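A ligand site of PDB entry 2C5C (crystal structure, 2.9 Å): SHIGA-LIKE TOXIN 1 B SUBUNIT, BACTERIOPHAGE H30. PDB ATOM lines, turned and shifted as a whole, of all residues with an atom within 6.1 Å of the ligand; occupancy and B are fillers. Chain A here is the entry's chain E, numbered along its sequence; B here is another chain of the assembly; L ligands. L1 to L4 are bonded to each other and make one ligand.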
ATOM      1  N   THR A   1      19.237   5.443 -14.346  1.00  0.00           N
ATOM      2  CA  THR A   1      18.580   5.752 -15.650  1.00  0.00           C
ATOM      3  C   THR A   1      18.845   7.179 -16.101  1.00  0.00           C
ATOM      4  O   THR A   1      18.791   8.080 -15.267  1.00  0.00           O
ATOM      5  CB  THR A   1      17.067   5.598 -15.445  1.00  0.00           C
ATOM      6  OG1 THR A   1      16.834   4.566 -14.519  1.00  0.00           O
ATOM      7  CG2 THR A   1      16.371   5.073 -16.657  1.00  0.00           C
ATOM      8  N   PHE A  30       4.592   7.455 -21.684  1.00  0.00           N
ATOM      9  CA  PHE A  30       3.566   6.788 -20.916  1.00  0.00           C
ATOM     10  C   PHE A  30       4.095   5.917 -19.845  1.00  0.00           C
ATOM     11  O   PHE A  30       5.230   5.546 -19.906  1.00  0.00           O
ATOM     12  CB  PHE A  30       2.729   5.930 -21.775  1.00  0.00           C
ATOM     13  CG  PHE A  30       3.343   4.631 -22.101  1.00  0.00           C
ATOM     14  CD1 PHE A  30       4.236   4.496 -23.174  1.00  0.00           C
ATOM     15  CD2 PHE A  30       2.958   3.498 -21.419  1.00  0.00           C
ATOM     16  CE1 PHE A  30       4.762   3.258 -23.517  1.00  0.00           C
ATOM     17  CE2 PHE A  30       3.468   2.229 -21.756  1.00  0.00           C
ATOM     18  CZ  PHE A  30       4.374   2.106 -22.798  1.00  0.00           C
ATOM     19  N   THR A  31       3.253   5.636 -18.846  1.00  0.00           N
ATOM     20  CA  THR A  31       3.605   4.792 -17.713  1.00  0.00           C
ATOM     21  C   THR A  31       2.458   3.955 -17.331  1.00  0.00           C
ATOM     22  O   THR A  31       1.347   4.430 -17.193  1.00  0.00           O
ATOM     23  CB  THR A  31       4.035   5.529 -16.499  1.00  0.00           C
ATOM     24  OG1 THR A  31       4.352   4.557 -15.480  1.00  0.00           O
ATOM     25  CG2 THR A  31       2.942   6.415 -15.872  1.00  0.00           C
ATOM     26  N   ASN A  32       2.774   2.685 -17.147  1.00  0.00           N
ATOM     27  CA  ASN A  32       1.860   1.665 -16.709  1.00  0.00           C
ATOM     28  C   ASN A  32       1.702   1.590 -15.178  1.00  0.00           C
ATOM     29  O   ASN A  32       0.966   0.756 -14.680  1.00  0.00           O
ATOM     30  CB  ASN A  32       2.281   0.304 -17.312  1.00  0.00           C
ATOM     31  CG  ASN A  32       3.460  -0.265 -16.684  1.00  0.00           C
ATOM     32  OD1 ASN A  32       4.200   0.383 -16.064  1.00  0.00           O
ATOM     33  ND2 ASN A  32       3.645  -1.508 -16.870  1.00  0.00           N
ATOM     34  N   ARG A  33       2.350   2.474 -14.441  1.00  0.00           N
ATOM     35  CA  ARG A  33       2.229   2.499 -12.969  1.00  0.00           C
ATOM     36  C   ARG A  33       1.044   3.356 -12.577  1.00  0.00           C
ATOM     37  O   ARG A  33       0.989   4.584 -12.886  1.00  0.00           O
ATOM     38  CB  ARG A  33       3.485   3.116 -12.351  1.00  0.00           C
ATOM     39  CG  ARG A  33       4.794   2.487 -12.762  1.00  0.00           C
ATOM     40  CD  ARG A  33       4.880   0.953 -12.633  1.00  0.00           C
ATOM     41  NE  ARG A  33       6.154   0.538 -13.210  1.00  0.00           N
ATOM     42  CZ  ARG A  33       7.316   0.415 -12.554  1.00  0.00           C
ATOM     43  NH1 ARG A  33       7.383   0.630 -11.279  1.00  0.00           N
ATOM     44  NH2 ARG A  33       8.419   0.088 -13.228  1.00  0.00           N
ATOM     45  N   LYS A  53      12.896  10.281 -16.113  1.00  0.00           N
ATOM     46  CA  LYS A  53      14.061   9.424 -16.380  1.00  0.00           C
ATOM     47  C   LYS A  53      13.644   8.191 -17.166  1.00  0.00           C
ATOM     48  O   LYS A  53      12.761   7.419 -16.697  1.00  0.00           O
ATOM     49  CB  LYS A  53      14.771   9.028 -15.067  1.00  0.00           C
ATOM     50  CG  LYS A  53      15.775  10.147 -14.532  1.00  0.00           C
ATOM     51  CD  LYS A  53      16.128   9.983 -13.048  1.00  0.00           C
ATOM     52  CE  LYS A  53      17.677  10.011 -12.719  1.00  0.00           C
ATOM     53  NZ  LYS A  53      18.533  10.983 -13.519  1.00  0.00           N
ATOM     54  N   THR A  54      14.204   8.023 -18.370  1.00  0.00           N
ATOM     55  CA  THR A  54      13.926   6.791 -19.128  1.00  0.00           C
ATOM     56  C   THR A  54      14.916   6.564 -20.215  1.00  0.00           C
ATOM     57  O   THR A  54      15.353   7.526 -20.817  1.00  0.00           O
ATOM     58  CB  THR A  54      12.496   6.755 -19.688  1.00  0.00           C
ATOM     59  OG1 THR A  54      12.273   5.537 -20.418  1.00  0.00           O
ATOM     60  CG2 THR A  54      12.334   7.851 -20.696  1.00  0.00           C
ATOM     61  N   ASN A  55      15.246   5.285 -20.445  1.00  0.00           N
ATOM     62  CA  ASN A  55      16.078   4.881 -21.600  1.00  0.00           C
ATOM     63  C   ASN A  55      15.299   4.882 -22.900  1.00  0.00           C
ATOM     64  O   ASN A  55      15.906   4.852 -23.938  1.00  0.00           O
ATOM     65  CB  ASN A  55      16.635   3.467 -21.458  1.00  0.00           C
ATOM     66  CG  ASN A  55      17.998   3.428 -20.854  1.00  0.00           C
ATOM     67  OD1 ASN A  55      18.155   2.752 -19.743  1.00  0.00           O
ATOM     68  ND2 ASN A  55      19.039   4.066 -21.557  1.00  0.00           N
ATOM     69  N   ALA A  56      13.961   4.892 -22.844  1.00  0.00           N
ATOM     70  CA  ALA A  56      13.148   4.875 -24.037  1.00  0.00           C
ATOM     71  C   ALA A  56      12.754   6.263 -24.352  1.00  0.00           C
ATOM     72  O   ALA A  56      11.578   6.580 -24.313  1.00  0.00           O
ATOM     73  CB  ALA A  56      11.900   4.001 -23.825  1.00  0.00           C
ATOM     74  N   HIS A  58      11.892   8.624 -26.481  1.00  0.00           N
ATOM     75  CA  HIS A  58      11.314   8.925 -27.766  1.00  0.00           C
ATOM     76  C   HIS A  58       9.811   9.058 -27.624  1.00  0.00           C
ATOM     77  O   HIS A  58       9.232   8.576 -26.686  1.00  0.00           O
ATOM     78  CB  HIS A  58      11.709   7.825 -28.764  1.00  0.00           C
ATOM     79  CG  HIS A  58      11.580   6.434 -28.243  1.00  0.00           C
ATOM     80  ND1 HIS A  58      10.364   5.778 -28.173  1.00  0.00           N
ATOM     81  CD2 HIS A  58      12.506   5.545 -27.795  1.00  0.00           C
ATOM     82  CE1 HIS A  58      10.544   4.560 -27.691  1.00  0.00           C
ATOM     83  NE2 HIS A  58      11.838   4.397 -27.446  1.00  0.00           N
ATOM     84  N   GLY A  61       7.333   6.356 -25.849  1.00  0.00           N
ATOM     85  CA  GLY A  61       8.212   5.530 -25.034  1.00  0.00           C
ATOM     86  C   GLY A  61       7.725   5.409 -23.640  1.00  0.00           C
ATOM     87  O   GLY A  61       6.995   6.257 -23.206  1.00  0.00           O
ATOM     88  N   GLY A  62       8.148   4.380 -22.925  1.00  0.00           N
ATOM     89  CA  GLY A  62       7.680   4.157 -21.558  1.00  0.00           C
ATOM     90  C   GLY A  62       8.552   4.745 -20.481  1.00  0.00           C
ATOM     91  O   GLY A  62       9.749   4.951 -20.672  1.00  0.00           O
ATOM     92  N   PHE A  63       7.957   5.000 -19.324  1.00  0.00           N
ATOM     93  CA  PHE A  63       8.718   5.481 -18.159  1.00  0.00           C
ATOM     94  C   PHE A  63       8.060   5.063 -16.904  1.00  0.00           C
ATOM     95  O   PHE A  63       6.848   4.760 -16.920  1.00  0.00           O
ATOM     96  CB  PHE A  63       8.846   7.001 -18.142  1.00  0.00           C
ATOM     97  CG  PHE A  63       7.566   7.734 -17.685  1.00  0.00           C
ATOM     98  CD1 PHE A  63       6.580   8.089 -18.631  1.00  0.00           C
ATOM     99  CD2 PHE A  63       7.394   8.154 -16.378  1.00  0.00           C
ATOM    100  CE1 PHE A  63       5.450   8.803 -18.266  1.00  0.00           C
ATOM    101  CE2 PHE A  63       6.257   8.845 -16.017  1.00  0.00           C
ATOM    102  CZ  PHE A  63       5.293   9.174 -16.950  1.00  0.00           C
ATOM    103  N   SER A  64       8.883   5.011 -15.846  1.00  0.00           N
ATOM    104  CA  SER A  64       8.417   4.832 -14.472  1.00  0.00           C
ATOM    105  C   SER A  64       9.113   5.690 -13.491  1.00  0.00           C
ATOM    106  O   SER A  64       8.705   5.678 -12.441  1.00  0.00           O
ATOM    107  CB  SER A  64       8.602   3.409 -14.027  1.00  0.00           C
ATOM    108  OG  SER A  64       9.942   3.155 -13.871  1.00  0.00           O
ATOM    109  N   GLU A  65      10.167   6.400 -13.817  1.00  0.00           N
ATOM    110  CA  GLU A  65      10.867   7.258 -12.868  1.00  0.00           C
ATOM    111  C   GLU A  65      10.571   8.735 -13.107  1.00  0.00           C
ATOM    112  O   GLU A  65      10.685   9.222 -14.216  1.00  0.00           O
ATOM    113  CB  GLU A  65      12.366   7.017 -12.952  1.00  0.00           C
ATOM    114  CG  GLU A  65      12.834   5.737 -12.293  1.00  0.00           C
ATOM    115  CD  GLU A  65      14.263   5.359 -12.657  1.00  0.00           C
ATOM    116  OE1 GLU A  65      15.273   6.069 -12.315  1.00  0.00           O
ATOM    117  OE2 GLU A  65      14.334   4.305 -13.329  1.00  0.00           O
ATOM    118  N   ASP B  16      11.951   3.145  -9.971  1.00  0.00           N
ATOM    119  CA  ASP B  16      11.566   2.114 -10.883  1.00  0.00           C
ATOM    120  C   ASP B  16      10.987   0.920 -10.209  1.00  0.00           C
ATOM    121  O   ASP B  16      10.217   0.283 -10.850  1.00  0.00           O
ATOM    122  CB  ASP B  16      12.694   1.719 -11.787  1.00  0.00           C
ATOM    123  CG  ASP B  16      12.292   0.616 -12.722  1.00  0.00           C
ATOM    124  OD1 ASP B  16      11.374   0.835 -13.586  1.00  0.00           O
ATOM    125  OD2 ASP B  16      12.813  -0.529 -12.592  1.00  0.00           O
HETATM  126  C1  LIG L   1      17.856  -2.019 -22.499  1.00  0.00           C
HETATM  127  C2  LIG L   1      17.569  -1.869 -20.995  1.00  0.00           C
HETATM  128  C3  LIG L   1      16.065  -1.839 -20.754  1.00  0.00           C
HETATM  129  C4  LIG L   1      15.245  -0.884 -21.611  1.00  0.00           C
HETATM  130  C5  LIG L   1      15.672  -1.141 -23.061  1.00  0.00           C
HETATM  131  C6  LIG L   1      14.980  -0.198 -24.071  1.00  0.00           C
HETATM  132  O1  LIG L   1      19.213  -1.992 -22.962  1.00  0.00           O
HETATM  133  O2  LIG L   1      17.846  -3.103 -20.401  1.00  0.00           O
HETATM  134  O3  LIG L   1      15.731  -1.760 -19.408  1.00  0.00           O
HETATM  135  O4  LIG L   1      13.853  -1.167 -21.467  1.00  0.00           O
HETATM  136  O5  LIG L   1      17.098  -0.989 -23.100  1.00  0.00           O
HETATM  137  O6  LIG L   1      15.303   1.119 -23.742  1.00  0.00           O
HETATM  138  C1  LG2 L   2      13.060   0.013 -21.460  1.00  0.00           C
HETATM  139  C2  LG2 L   2      11.558  -0.256 -21.612  1.00  0.00           C
HETATM  140  C3  LG2 L   2      10.667   0.973 -21.415  1.00  0.00           C
HETATM  141  C4  LG2 L   2      10.894   1.667 -20.033  1.00  0.00           C
HETATM  142  C5  LG2 L   2      12.428   1.772 -19.873  1.00  0.00           C
HETATM  143  C6  LG2 L   2      12.836   2.431 -18.572  1.00  0.00           C
HETATM  144  O1  LG2 L   2      11.123  -1.098 -22.641  1.00  0.00           O
HETATM  145  O2  LG2 L   2       9.348   0.456 -21.467  1.00  0.00           O
HETATM  146  O3  LG2 L   2      10.360   0.880 -18.972  1.00  0.00           O
HETATM  147  O4  LG2 L   2      13.267   0.572 -20.155  1.00  0.00           O
HETATM  148  O5  LG2 L   2      13.905   3.278 -18.995  1.00  0.00           O
HETATM  149  C1  LG3 L   3       9.630   1.505 -17.882  1.00  0.00           C
HETATM  150  C2  LG3 L   3       9.675   0.619 -16.582  1.00  0.00           C
HETATM  151  C3  LG3 L   3       8.869  -0.584 -16.802  1.00  0.00           C
HETATM  152  C4  LG3 L   3       7.502  -0.137 -17.158  1.00  0.00           C
HETATM  153  C5  LG3 L   3       7.437   0.853 -18.368  1.00  0.00           C
HETATM  154  C6  LG3 L   3       6.006   1.332 -18.737  1.00  0.00           C
HETATM  155  O1  LG3 L   3      10.949   0.051 -16.365  1.00  0.00           O
HETATM  156  O2  LG3 L   3       8.759  -1.363 -15.646  1.00  0.00           O
HETATM  157  O3  LG3 L   3       6.984   0.189 -15.912  1.00  0.00           O
HETATM  158  O4  LG3 L   3       8.298   1.938 -18.194  1.00  0.00           O
HETATM  159  O5  LG3 L   3       5.677   2.362 -17.831  1.00  0.00           O
HETATM  160  O1  LG4 L   4       5.777  -2.094 -24.280  1.00  0.00           O
HETATM  161  C1  LG4 L   4       6.258  -1.763 -23.143  1.00  0.00           C
HETATM  162  O2  LG4 L   4       7.736  -1.871 -22.761  1.00  0.00           O
HETATM  163  C2  LG4 L   4       8.824  -2.714 -23.327  1.00  0.00           C
HETATM  164  C3  LG4 L   4      10.216  -2.276 -22.825  1.00  0.00           C
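An oxygen (O5) of LG3 L3 lies within hydrogen-bond range of the backbone NH (N) of Asn 32 (3.0 Å). The side-chain amide oxygen (OD1) of Asn 32 sits at hydrogen-bond distance from an oxygen (O3) of LG3 L3, 2.8 Å away. The backbone NH (N) of Asn 55 lies within hydrogen-bond range of an oxygen (O5) of LG2 L2 (2.8 Å). The backbone NH (N) of Phe 63 sits at hydrogen-bond distance from an oxygen (O4) of LG3 L3, at 3.3 Å. An oxygen (O5) of LG3 L3 sits at hydrogen-bond distance from the backbone carbonyl oxygen (O) of Phe 63. O2 of LG3 L3 sits at hydrogen-bond distance from NH2 of Arg 33, 2.8 Å away. OD1 of Asp 16 of chain B lies within hydrogen-bond range of O1 of LG3 L3 (2.9 Å). The side-chain hydroxyl (OG1) of Thr 54 lies within hydrogen-bond range of an oxygen (O5) of LG2 L2, at 3.1 Å. The side-chain hydroxyl (OG1) of Thr 31 lies close to an oxygen (O5) of LG3 L3.
OD1 of Asn 32 lies within hydrogen-bond range of NE of Arg 33 (3.5 Å). The backbone NH (N) of Phe 63 is in hydrogen-bond range of the backbone carbonyl oxygen (O) of Phe 30, 2.8 Å away. The guanidinium group of Arg 33 is in salt-bridge range of the side-chain carboxylate of Asp 16 of chain B, at 3.1 Å. The side-chain hydroxyl of Ser 64 sits at hydrogen-bond distance from the side-chain carboxylate of Asp 16 of chain B. The backbone carbonyl oxygen (O) of Gly 62 lies within hydrogen-bond range of the side-chain hydroxyl (OG1) of Thr 54. The side-chain hydroxyl of Thr 54 lies within hydrogen-bond range of the backbone NH of Ala 56 (3.0 Å). N of Phe 30 is in hydrogen-bond range of O of Gly 61 (3.1 Å). O of Thr 1 lies close to NZ of Lys 53, at 3.4 Å.
Merely in contact with the ligand: Gly 62 (3.5 Å), Ser 64 (3.7 Å), Phe 30 (3.8 Å) and Thr 1 (3.8 Å). The nearest printed residue that does not touch the ligand is Ala 56 (4.1 Å).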
